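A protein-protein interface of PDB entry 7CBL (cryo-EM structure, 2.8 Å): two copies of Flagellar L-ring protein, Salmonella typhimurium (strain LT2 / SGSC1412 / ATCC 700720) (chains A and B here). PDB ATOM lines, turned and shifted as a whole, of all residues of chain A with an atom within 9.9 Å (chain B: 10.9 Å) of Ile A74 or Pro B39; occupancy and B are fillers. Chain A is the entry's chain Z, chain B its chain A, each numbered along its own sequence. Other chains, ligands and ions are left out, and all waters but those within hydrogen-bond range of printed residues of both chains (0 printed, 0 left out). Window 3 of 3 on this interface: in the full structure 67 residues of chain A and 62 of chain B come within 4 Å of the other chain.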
ATOM      1  N   TYR A  60     -20.207 -23.095 -10.462  1.00  0.00           N
ATOM      2  CA  TYR A  60     -19.776 -21.722 -10.270  1.00  0.00           C
ATOM      3  C   TYR A  60     -20.824 -20.785 -10.855  1.00  0.00           C
ATOM      4  O   TYR A  60     -21.658 -21.180 -11.672  1.00  0.00           O
ATOM      5  CB  TYR A  60     -18.408 -21.488 -10.912  1.00  0.00           C
ATOM      6  CG  TYR A  60     -17.405 -22.562 -10.564  1.00  0.00           C
ATOM      7  CD1 TYR A  60     -17.335 -23.080  -9.280  1.00  0.00           C
ATOM      8  CD2 TYR A  60     -16.535 -23.066 -11.519  1.00  0.00           C
ATOM      9  CE1 TYR A  60     -16.431 -24.066  -8.955  1.00  0.00           C
ATOM     10  CE2 TYR A  60     -15.624 -24.055 -11.201  1.00  0.00           C
ATOM     11  CZ  TYR A  60     -15.577 -24.550  -9.917  1.00  0.00           C
ATOM     12  OH  TYR A  60     -14.676 -25.533  -9.586  1.00  0.00           O
ATOM     13  N   ARG A  70     -11.695  -9.987 -15.688  1.00  0.00           N
ATOM     14  CA  ARG A  70     -11.289  -9.159 -14.573  1.00  0.00           C
ATOM     15  C   ARG A  70     -11.578  -9.871 -13.262  1.00  0.00           C
ATOM     16  O   ARG A  70     -12.503 -10.681 -13.183  1.00  0.00           O
ATOM     17  CB  ARG A  70     -12.034  -7.826 -14.583  1.00  0.00           C
ATOM     18  CG  ARG A  70     -11.689  -6.923 -15.735  1.00  0.00           C
ATOM     19  CD  ARG A  70     -12.629  -5.744 -15.770  1.00  0.00           C
ATOM     20  NE  ARG A  70     -12.310  -4.818 -16.847  1.00  0.00           N
ATOM     21  CZ  ARG A  70     -13.028  -3.740 -17.132  1.00  0.00           C
ATOM     22  NH1 ARG A  70     -14.106  -3.455 -16.419  1.00  0.00           N
ATOM     23  NH2 ARG A  70     -12.669  -2.948 -18.128  1.00  0.00           N
ATOM     24  N   PRO A  71     -10.796  -9.607 -12.223  1.00  0.00           N
ATOM     25  CA  PRO A  71     -11.150 -10.117 -10.897  1.00  0.00           C
ATOM     26  C   PRO A  71     -12.410  -9.442 -10.385  1.00  0.00           C
ATOM     27  O   PRO A  71     -12.584  -8.230 -10.521  1.00  0.00           O
ATOM     28  CB  PRO A  71      -9.932  -9.761 -10.042  1.00  0.00           C
ATOM     29  CG  PRO A  71      -9.251  -8.681 -10.782  1.00  0.00           C
ATOM     30  CD  PRO A  71      -9.491  -8.936 -12.224  1.00  0.00           C
ATOM     31  N   ARG A  72     -13.300 -10.239  -9.805  1.00  0.00           N
ATOM     32  CA  ARG A  72     -14.582  -9.733  -9.339  1.00  0.00           C
ATOM     33  C   ARG A  72     -14.912 -10.076  -7.899  1.00  0.00           C
ATOM     34  O   ARG A  72     -15.701  -9.351  -7.287  1.00  0.00           O
ATOM     35  CB  ARG A  72     -15.721 -10.248 -10.228  1.00  0.00           C
ATOM     36  CG  ARG A  72     -15.563  -9.899 -11.689  1.00  0.00           C
ATOM     37  CD  ARG A  72     -16.680 -10.489 -12.516  1.00  0.00           C
ATOM     38  NE  ARG A  72     -16.209 -10.907 -13.831  1.00  0.00           N
ATOM     39  CZ  ARG A  72     -16.161 -10.112 -14.892  1.00  0.00           C
ATOM     40  NH1 ARG A  72     -16.561  -8.854 -14.796  1.00  0.00           N
ATOM     41  NH2 ARG A  72     -15.715 -10.575 -16.050  1.00  0.00           N
ATOM     42  N   ASN A  73     -14.354 -11.143  -7.337  1.00  0.00           N
ATOM     43  CA  ASN A  73     -14.674 -11.558  -5.984  1.00  0.00           C
ATOM     44  C   ASN A  73     -13.395 -11.794  -5.199  1.00  0.00           C
ATOM     45  O   ASN A  73     -12.289 -11.741  -5.736  1.00  0.00           O
ATOM     46  CB  ASN A  73     -15.528 -12.827  -5.974  1.00  0.00           C
ATOM     47  CG  ASN A  73     -16.841 -12.645  -6.682  1.00  0.00           C
ATOM     48  OD1 ASN A  73     -17.787 -12.092  -6.124  1.00  0.00           O
ATOM     49  ND2 ASN A  73     -16.914 -13.113  -7.919  1.00  0.00           N
ATOM     50  N   ILE A  74     -13.568 -12.060  -3.905  1.00  0.00           N
ATOM     51  CA  ILE A  74     -12.436 -12.374  -3.049  1.00  0.00           C
ATOM     52  C   ILE A  74     -11.799 -13.670  -3.515  1.00  0.00           C
ATOM     53  O   ILE A  74     -12.481 -14.684  -3.703  1.00  0.00           O
ATOM     54  CB  ILE A  74     -12.890 -12.472  -1.587  1.00  0.00           C
ATOM     55  CG1 ILE A  74     -13.286 -11.098  -1.063  1.00  0.00           C
ATOM     56  CG2 ILE A  74     -11.801 -13.071  -0.737  1.00  0.00           C
ATOM     57  CD1 ILE A  74     -13.697 -11.102   0.375  1.00  0.00           C
ATOM     58  N   GLY A  75     -10.487 -13.643  -3.712  1.00  0.00           N
ATOM     59  CA  GLY A  75      -9.741 -14.816  -4.108  1.00  0.00           C
ATOM     60  C   GLY A  75      -9.282 -14.823  -5.545  1.00  0.00           C
ATOM     61  O   GLY A  75      -8.510 -15.711  -5.920  1.00  0.00           O
ATOM     62  N   ASP A  76      -9.726 -13.880  -6.363  1.00  0.00           N
ATOM     63  CA  ASP A  76      -9.305 -13.832  -7.751  1.00  0.00           C
ATOM     64  C   ASP A  76      -7.905 -13.247  -7.863  1.00  0.00           C
ATOM     65  O   ASP A  76      -7.478 -12.443  -7.036  1.00  0.00           O
ATOM     66  CB  ASP A  76     -10.280 -12.998  -8.576  1.00  0.00           C
ATOM     67  CG  ASP A  76     -11.603 -13.694  -8.790  1.00  0.00           C
ATOM     68  OD1 ASP A  76     -12.611 -13.235  -8.219  1.00  0.00           O
ATOM     69  OD2 ASP A  76     -11.639 -14.701  -9.525  1.00  0.00           O
ATOM     70  N   THR A  77      -7.193 -13.652  -8.905  1.00  0.00           N
ATOM     71  CA  THR A  77      -5.812 -13.244  -9.102  1.00  0.00           C
ATOM     72  C   THR A  77      -5.720 -12.132 -10.138  1.00  0.00           C
ATOM     73  O   THR A  77      -6.601 -11.960 -10.980  1.00  0.00           O
ATOM     74  CB  THR A  77      -4.954 -14.432  -9.537  1.00  0.00           C
ATOM     75  OG1 THR A  77      -5.202 -14.717 -10.916  1.00  0.00           O
ATOM     76  CG2 THR A  77      -5.292 -15.653  -8.712  1.00  0.00           C
ATOM     77  N   VAL A 150      -0.964 -10.903  -7.691  1.00  0.00           N
ATOM     78  CA  VAL A 150      -1.549 -10.682  -6.379  1.00  0.00           C
ATOM     79  C   VAL A 150      -2.971 -11.217  -6.357  1.00  0.00           C
ATOM     80  O   VAL A 150      -3.497 -11.652  -7.385  1.00  0.00           O
ATOM     81  CB  VAL A 150      -1.524  -9.192  -6.013  1.00  0.00           C
ATOM     82  CG1 VAL A 150      -0.106  -8.687  -5.989  1.00  0.00           C
ATOM     83  CG2 VAL A 150      -2.335  -8.414  -7.009  1.00  0.00           C
ATOM     84  N   THR A 151      -3.605 -11.166  -5.195  1.00  0.00           N
ATOM     85  CA  THR A 151      -4.919 -11.741  -4.971  1.00  0.00           C
ATOM     86  C   THR A 151      -5.820 -10.700  -4.328  1.00  0.00           C
ATOM     87  O   THR A 151      -5.368  -9.904  -3.498  1.00  0.00           O
ATOM     88  CB  THR A 151      -4.820 -12.977  -4.072  1.00  0.00           C
ATOM     89  OG1 THR A 151      -3.922 -13.920  -4.660  1.00  0.00           O
ATOM     90  CG2 THR A 151      -6.166 -13.633  -3.903  1.00  0.00           C
ATOM     91  N   VAL A 152      -7.087 -10.704  -4.721  1.00  0.00           N
ATOM     92  CA  VAL A 152      -8.080  -9.810  -4.142  1.00  0.00           C
ATOM     93  C   VAL A 152      -8.476 -10.338  -2.775  1.00  0.00           C
ATOM     94  O   VAL A 152      -8.833 -11.512  -2.633  1.00  0.00           O
ATOM     95  CB  VAL A 152      -9.305  -9.694  -5.059  1.00  0.00           C
ATOM     96  CG1 VAL A 152     -10.348  -8.809  -4.426  1.00  0.00           C
ATOM     97  CG2 VAL A 152      -8.904  -9.166  -6.411  1.00  0.00           C
ATOM     98  N   ASP A 153      -8.424  -9.479  -1.761  1.00  0.00           N
ATOM     99  CA  ASP A 153      -8.816  -9.874  -0.421  1.00  0.00           C
ATOM    100  C   ASP A 153     -10.016  -9.107   0.103  1.00  0.00           C
ATOM    101  O   ASP A 153     -10.512  -9.433   1.186  1.00  0.00           O
ATOM    102  CB  ASP A 153      -7.647  -9.706   0.553  1.00  0.00           C
ATOM    103  CG  ASP A 153      -7.381  -8.266   0.889  1.00  0.00           C
ATOM    104  OD1 ASP A 153      -6.851  -7.544   0.025  1.00  0.00           O
ATOM    105  OD2 ASP A 153      -7.695  -7.849   2.023  1.00  0.00           O
ATOM    106  N   GLN A 154     -10.501  -8.107  -0.624  1.00  0.00           N
ATOM    107  CA  GLN A 154     -11.682  -7.369  -0.206  1.00  0.00           C
ATOM    108  C   GLN A 154     -12.201  -6.569  -1.386  1.00  0.00           C
ATOM    109  O   GLN A 154     -11.423  -6.082  -2.208  1.00  0.00           O
ATOM    110  CB  GLN A 154     -11.375  -6.439   0.969  1.00  0.00           C
ATOM    111  CG  GLN A 154     -12.604  -5.835   1.599  1.00  0.00           C
ATOM    112  CD  GLN A 154     -12.270  -4.738   2.574  1.00  0.00           C
ATOM    113  OE1 GLN A 154     -11.108  -4.531   2.916  1.00  0.00           O
ATOM    114  NE2 GLN A 154     -13.288  -4.020   3.029  1.00  0.00           N
ATOM    115  N   VAL A 155     -13.521  -6.445  -1.463  1.00  0.00           N
ATOM    116  CA  VAL A 155     -14.185  -5.628  -2.470  1.00  0.00           C
ATOM    117  C   VAL A 155     -14.813  -4.443  -1.756  1.00  0.00           C
ATOM    118  O   VAL A 155     -15.651  -4.618  -0.865  1.00  0.00           O
ATOM    119  CB  VAL A 155     -15.237  -6.425  -3.251  1.00  0.00           C
ATOM    120  CG1 VAL A 155     -15.795  -5.587  -4.373  1.00  0.00           C
ATOM    121  CG2 VAL A 155     -14.632  -7.694  -3.798  1.00  0.00           C
ATOM    122  N   LEU A 156     -14.409  -3.240  -2.143  1.00  0.00           N
ATOM    123  CA  LEU A 156     -14.859  -2.045  -1.455  1.00  0.00           C
ATOM    124  C   LEU A 156     -16.264  -1.661  -1.910  1.00  0.00           C
ATOM    125  O   LEU A 156     -16.825  -2.230  -2.847  1.00  0.00           O
ATOM    126  CB  LEU A 156     -13.879  -0.902  -1.688  1.00  0.00           C
ATOM    127  CG  LEU A 156     -12.426  -1.252  -1.383  1.00  0.00           C
ATOM    128  CD1 LEU A 156     -11.536  -0.054  -1.592  1.00  0.00           C
ATOM    129  CD2 LEU A 156     -12.299  -1.767   0.030  1.00  0.00           C
ATOM    130  N   ASN A 160     -13.989  -0.915  -6.040  1.00  0.00           N
ATOM    131  CA  ASN A 160     -12.544  -1.043  -6.002  1.00  0.00           C
ATOM    132  C   ASN A 160     -12.145  -2.328  -5.288  1.00  0.00           C
ATOM    133  O   ASN A 160     -12.876  -2.858  -4.449  1.00  0.00           O
ATOM    134  CB  ASN A 160     -11.914   0.157  -5.303  1.00  0.00           C
ATOM    135  CG  ASN A 160     -12.061   1.432  -6.096  1.00  0.00           C
ATOM    136  OD1 ASN A 160     -12.345   2.489  -5.542  1.00  0.00           O
ATOM    137  ND2 ASN A 160     -11.869   1.340  -7.400  1.00  0.00           N
ATOM    138  N   LEU A 161     -10.965  -2.831  -5.631  1.00  0.00           N
ATOM    139  CA  LEU A 161     -10.475  -4.101  -5.120  1.00  0.00           C
ATOM    140  C   LEU A 161      -9.216  -3.873  -4.304  1.00  0.00           C
ATOM    141  O   LEU A 161      -8.254  -3.287  -4.801  1.00  0.00           O
ATOM    142  CB  LEU A 161     -10.175  -5.071  -6.260  1.00  0.00           C
ATOM    143  CG  LEU A 161     -11.224  -5.247  -7.351  1.00  0.00           C
ATOM    144  CD1 LEU A 161     -10.567  -5.758  -8.609  1.00  0.00           C
ATOM    145  CD2 LEU A 161     -12.302  -6.198  -6.894  1.00  0.00           C
ATOM    146  N   HIS A 162      -9.214  -4.341  -3.064  1.00  0.00           N
ATOM    147  CA  HIS A 162      -8.002  -4.356  -2.260  1.00  0.00           C
ATOM    148  C   HIS A 162      -7.231  -5.634  -2.556  1.00  0.00           C
ATOM    149  O   HIS A 162      -7.784  -6.731  -2.456  1.00  0.00           O
ATOM    150  CB  HIS A 162      -8.337  -4.261  -0.775  1.00  0.00           C
ATOM    151  CG  HIS A 162      -7.141  -4.056   0.094  1.00  0.00           C
ATOM    152  ND1 HIS A 162      -6.687  -5.017   0.970  1.00  0.00           N
ATOM    153  CD2 HIS A 162      -6.296  -3.008   0.214  1.00  0.00           C
ATOM    154  CE1 HIS A 162      -5.615  -4.567   1.595  1.00  0.00           C
ATOM    155  NE2 HIS A 162      -5.357  -3.349   1.155  1.00  0.00           N
ATOM    156  N   VAL A 163      -5.963  -5.495  -2.933  1.00  0.00           N
ATOM    157  CA  VAL A 163      -5.155  -6.617  -3.387  1.00  0.00           C
ATOM    158  C   VAL A 163      -3.913  -6.733  -2.519  1.00  0.00           C
ATOM    159  O   VAL A 163      -3.341  -5.722  -2.093  1.00  0.00           O
ATOM    160  CB  VAL A 163      -4.764  -6.481  -4.873  1.00  0.00           C
ATOM    161  CG1 VAL A 163      -5.992  -6.510  -5.741  1.00  0.00           C
ATOM    162  CG2 VAL A 163      -3.991  -5.212  -5.107  1.00  0.00           C
ATOM    163  N   VAL A 164      -3.502  -7.974  -2.259  1.00  0.00           N
ATOM    164  CA  VAL A 164      -2.285  -8.276  -1.518  1.00  0.00           C
ATOM    165  C   VAL A 164      -1.566  -9.412  -2.221  1.00  0.00           C
ATOM    166  O   VAL A 164      -2.188 -10.255  -2.868  1.00  0.00           O
ATOM    167  CB  VAL A 164      -2.571  -8.661  -0.056  1.00  0.00           C
ATOM    168  CG1 VAL A 164      -2.956  -7.443   0.744  1.00  0.00           C
ATOM    169  CG2 VAL A 164      -3.664  -9.698   0.000  1.00  0.00           C
ATOM    170  N   ALA B  34      -1.868 -11.159   6.396  1.00  0.00           N
ATOM    171  CA  ALA B  34      -1.791 -12.269   5.460  1.00  0.00           C
ATOM    172  C   ALA B  34      -1.731 -11.752   4.032  1.00  0.00           C
ATOM    173  O   ALA B  34      -2.449 -10.821   3.660  1.00  0.00           O
ATOM    174  CB  ALA B  34      -2.989 -13.197   5.634  1.00  0.00           C
ATOM    175  N   THR B  35      -0.864 -12.362   3.228  1.00  0.00           N
ATOM    176  CA  THR B  35      -0.686 -11.988   1.828  1.00  0.00           C
ATOM    177  C   THR B  35      -1.353 -12.980   0.891  1.00  0.00           C
ATOM    178  O   THR B  35      -0.837 -13.278  -0.187  1.00  0.00           O
ATOM    179  CB  THR B  35       0.794 -11.857   1.498  1.00  0.00           C
ATOM    180  OG1 THR B  35       1.466 -13.072   1.847  1.00  0.00           O
ATOM    181  CG2 THR B  35       1.407 -10.708   2.270  1.00  0.00           C
ATOM    182  N   THR B  36      -2.505 -13.509   1.287  1.00  0.00           N
ATOM    183  CA  THR B  36      -3.250 -14.437   0.452  1.00  0.00           C
ATOM    184  C   THR B  36      -4.695 -14.446   0.920  1.00  0.00           C
ATOM    185  O   THR B  36      -4.999 -14.087   2.060  1.00  0.00           O
ATOM    186  CB  THR B  36      -2.656 -15.847   0.504  1.00  0.00           C
ATOM    187  OG1 THR B  36      -3.367 -16.697  -0.401  1.00  0.00           O
ATOM    188  CG2 THR B  36      -2.760 -16.413   1.905  1.00  0.00           C
ATOM    189  N   ALA B  37      -5.583 -14.856   0.020  1.00  0.00           N
ATOM    190  CA  ALA B  37      -7.004 -14.916   0.314  1.00  0.00           C
ATOM    191  C   ALA B  37      -7.575 -16.210  -0.239  1.00  0.00           C
ATOM    192  O   ALA B  37      -7.074 -16.759  -1.220  1.00  0.00           O
ATOM    193  CB  ALA B  37      -7.755 -13.720  -0.273  1.00  0.00           C
ATOM    194  N   GLN B  38      -8.633 -16.689   0.401  1.00  0.00           N
ATOM    195  CA  GLN B  38      -9.260 -17.937   0.018  1.00  0.00           C
ATOM    196  C   GLN B  38     -10.584 -17.668  -0.670  1.00  0.00           C
ATOM    197  O   GLN B  38     -11.421 -16.941  -0.123  1.00  0.00           O
ATOM    198  CB  GLN B  38      -9.489 -18.817   1.247  1.00  0.00           C
ATOM    199  CG  GLN B  38      -8.320 -19.711   1.580  1.00  0.00           C
ATOM    200  CD  GLN B  38      -8.105 -20.782   0.533  1.00  0.00           C
ATOM    201  OE1 GLN B  38      -6.993 -20.971   0.041  1.00  0.00           O
ATOM    202  NE2 GLN B  38      -9.171 -21.491   0.185  1.00  0.00           N
ATOM    203  N   PRO B  39     -10.812 -18.228  -1.854  1.00  0.00           N
ATOM    204  CA  PRO B  39     -12.114 -18.065  -2.501  1.00  0.00           C
ATOM    205  C   PRO B  39     -13.204 -18.738  -1.689  1.00  0.00           C
ATOM    206  O   PRO B  39     -12.996 -19.782  -1.069  1.00  0.00           O
ATOM    207  CB  PRO B  39     -11.928 -18.750  -3.857  1.00  0.00           C
ATOM    208  CG  PRO B  39     -10.461 -18.872  -4.034  1.00  0.00           C
ATOM    209  CD  PRO B  39      -9.894 -19.028  -2.672  1.00  0.00           C
ATOM    210  N   ILE B  40     -14.378 -18.121  -1.696  1.00  0.00           N
ATOM    211  CA  ILE B  40     -15.524 -18.599  -0.928  1.00  0.00           C
ATOM    212  C   ILE B  40     -16.508 -19.263  -1.884  1.00  0.00           C
ATOM    213  O   ILE B  40     -16.735 -18.747  -2.987  1.00  0.00           O
ATOM    214  CB  ILE B  40     -16.184 -17.447  -0.159  1.00  0.00           C
ATOM    215  CG1 ILE B  40     -15.109 -16.549   0.454  1.00  0.00           C
ATOM    216  CG2 ILE B  40     -17.114 -17.983   0.916  1.00  0.00           C
ATOM    217  CD1 ILE B  40     -15.402 -16.086   1.859  1.00  0.00           C
ATOM    218  N   PRO B  41     -17.098 -20.403  -1.525  1.00  0.00           N
ATOM    219  CA  PRO B  41     -18.063 -21.043  -2.427  1.00  0.00           C
ATOM    220  C   PRO B  41     -19.302 -20.186  -2.624  1.00  0.00           C
ATOM    221  O   PRO B  41     -19.835 -19.601  -1.679  1.00  0.00           O
ATOM    222  CB  PRO B  41     -18.400 -22.357  -1.714  1.00  0.00           C
ATOM    223  CG  PRO B  41     -17.265 -22.594  -0.791  1.00  0.00           C
ATOM    224  CD  PRO B  41     -16.797 -21.245  -0.358  1.00  0.00           C
ATOM    225  N   GLY B  42     -19.762 -20.121  -3.871  1.00  0.00           N
ATOM    226  CA  GLY B  42     -20.945 -19.372  -4.216  1.00  0.00           C
ATOM    227  C   GLY B  42     -22.196 -19.950  -3.588  1.00  0.00           C
ATOM    228  O   GLY B  42     -22.206 -21.082  -3.096  1.00  0.00           O
ATOM    229  N   PRO B  43     -23.279 -19.178  -3.592  1.00  0.00           N
ATOM    230  CA  PRO B  43     -24.523 -19.645  -2.973  1.00  0.00           C
ATOM    231  C   PRO B  43     -25.151 -20.772  -3.777  1.00  0.00           C
ATOM    232  O   PRO B  43     -24.877 -20.967  -4.962  1.00  0.00           O
ATOM    233  CB  PRO B  43     -25.418 -18.401  -2.972  1.00  0.00           C
ATOM    234  CG  PRO B  43     -24.508 -17.251  -3.293  1.00  0.00           C
ATOM    235  CD  PRO B  43     -23.411 -17.817  -4.128  1.00  0.00           C
ATOM    236  N   ALA B  55     -25.447 -14.193  -7.951  1.00  0.00           N
ATOM    237  CA  ALA B  55     -25.159 -13.937  -6.548  1.00  0.00           C
ATOM    238  C   ALA B  55     -25.504 -12.493  -6.210  1.00  0.00           C
ATOM    239  O   ALA B  55     -25.484 -11.615  -7.075  1.00  0.00           O
ATOM    240  CB  ALA B  55     -23.688 -14.217  -6.241  1.00  0.00           C
ATOM    241  N   ILE B  58     -23.977  -6.117  -5.403  1.00  0.00           N
ATOM    242  CA  ILE B  58     -23.943  -4.834  -4.712  1.00  0.00           C
ATOM    243  C   ILE B  58     -24.291  -3.753  -5.727  1.00  0.00           C
ATOM    244  O   ILE B  58     -23.500  -3.453  -6.625  1.00  0.00           O
ATOM    245  CB  ILE B  58     -22.583  -4.575  -4.062  1.00  0.00           C
ATOM    246  CG1 ILE B  58     -22.093  -5.828  -3.338  1.00  0.00           C
ATOM    247  CG2 ILE B  58     -22.682  -3.414  -3.089  1.00  0.00           C
ATOM    248  CD1 ILE B  58     -23.037  -6.327  -2.269  1.00  0.00           C
ATOM    249  N   TYR B  60     -24.436  -0.485  -7.404  1.00  0.00           N
ATOM    250  CA  TYR B  60     -23.798   0.818  -7.448  1.00  0.00           C
ATOM    251  C   TYR B  60     -24.688   1.783  -8.220  1.00  0.00           C
ATOM    252  O   TYR B  60     -25.574   1.379  -8.974  1.00  0.00           O
ATOM    253  CB  TYR B  60     -22.412   0.722  -8.085  1.00  0.00           C
ATOM    254  CG  TYR B  60     -21.585  -0.411  -7.525  1.00  0.00           C
ATOM    255  CD1 TYR B  60     -21.595  -0.694  -6.167  1.00  0.00           C
ATOM    256  CD2 TYR B  60     -20.806  -1.206  -8.351  1.00  0.00           C
ATOM    257  CE1 TYR B  60     -20.853  -1.731  -5.648  1.00  0.00           C
ATOM    258  CE2 TYR B  60     -20.058  -2.248  -7.837  1.00  0.00           C
ATOM    259  CZ  TYR B  60     -20.086  -2.505  -6.484  1.00  0.00           C
ATOM    260  OH  TYR B  60     -19.347  -3.538  -5.960  1.00  0.00           O
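The backbone NH of Gly A75 sits at hydrogen-bond distance from the backbone carbonyl oxygen of Val A152 (2.9 Å).
The backbone NH of Val A152 is in hydrogen-bond range of the backbone carbonyl oxygen of Asp A76.
The backbone carbonyl oxygen of Val A164 is in hydrogen-bond range of the backbone NH of Thr A151 (2.9 Å).
OD1 of Asp A153 sits at hydrogen-bond distance from ND1 of His A162 (2.7 Å).
CG2 of Ile A74 touches O of Gln B38, 3.9 Å away.
Ile A74 touches Pro B39 (O to CA, 3.6 Å).
Ala B37 touches Thr A151 (CB to CG2, 3.96 Å).
Val A152 touches Ala B37.
CA of Asp A153 touches CB of Ala B37, at 3.99 Å.
No residue of chain B comes within 4 Å of Asn A73.
Ile A74 touches just these residues of chain B: Gln B38 (3.9 Å) and Pro B39 (3.6 Å).
Asp A76 touches none of the printed residues of chain B.
Of the printed residues of chain B, Thr A151 touches Ala B37.
Val A152 touches just one residue of chain B: Ala B37 (3.4 Å).
Printed residues of chain B within 4 Å of Asp A153: Ala B37.
Of the printed residues of chain A, Ala B37 touches Thr A151, Val A152 and Asp A153.
Of the printed residues of chain A, Pro B39 touches Ile A74.
Ile B40 touches none of the printed residues of chain A.
Of the 13 printed residues of chain B, 3 touch a printed residue of chain A.
Printed residues of chain B that touch a printed residue of chain A: Ala B37, Gln B38 and Pro B39.
Hydrophobic or aromatic side chains of chain B within 4 Å of the printed part of chain A: Ala B37.
Hydrophobic or aromatic side chains of chain A within 4 Å of the printed part of chain B: Ile A74.
Among the printed residues, 5 pairs touch across the chains.
Position printed for both chains: 60.
Of the 5 pairs that touch across the chains among the printed residues, none has its exchanged pair printed and touching as well.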
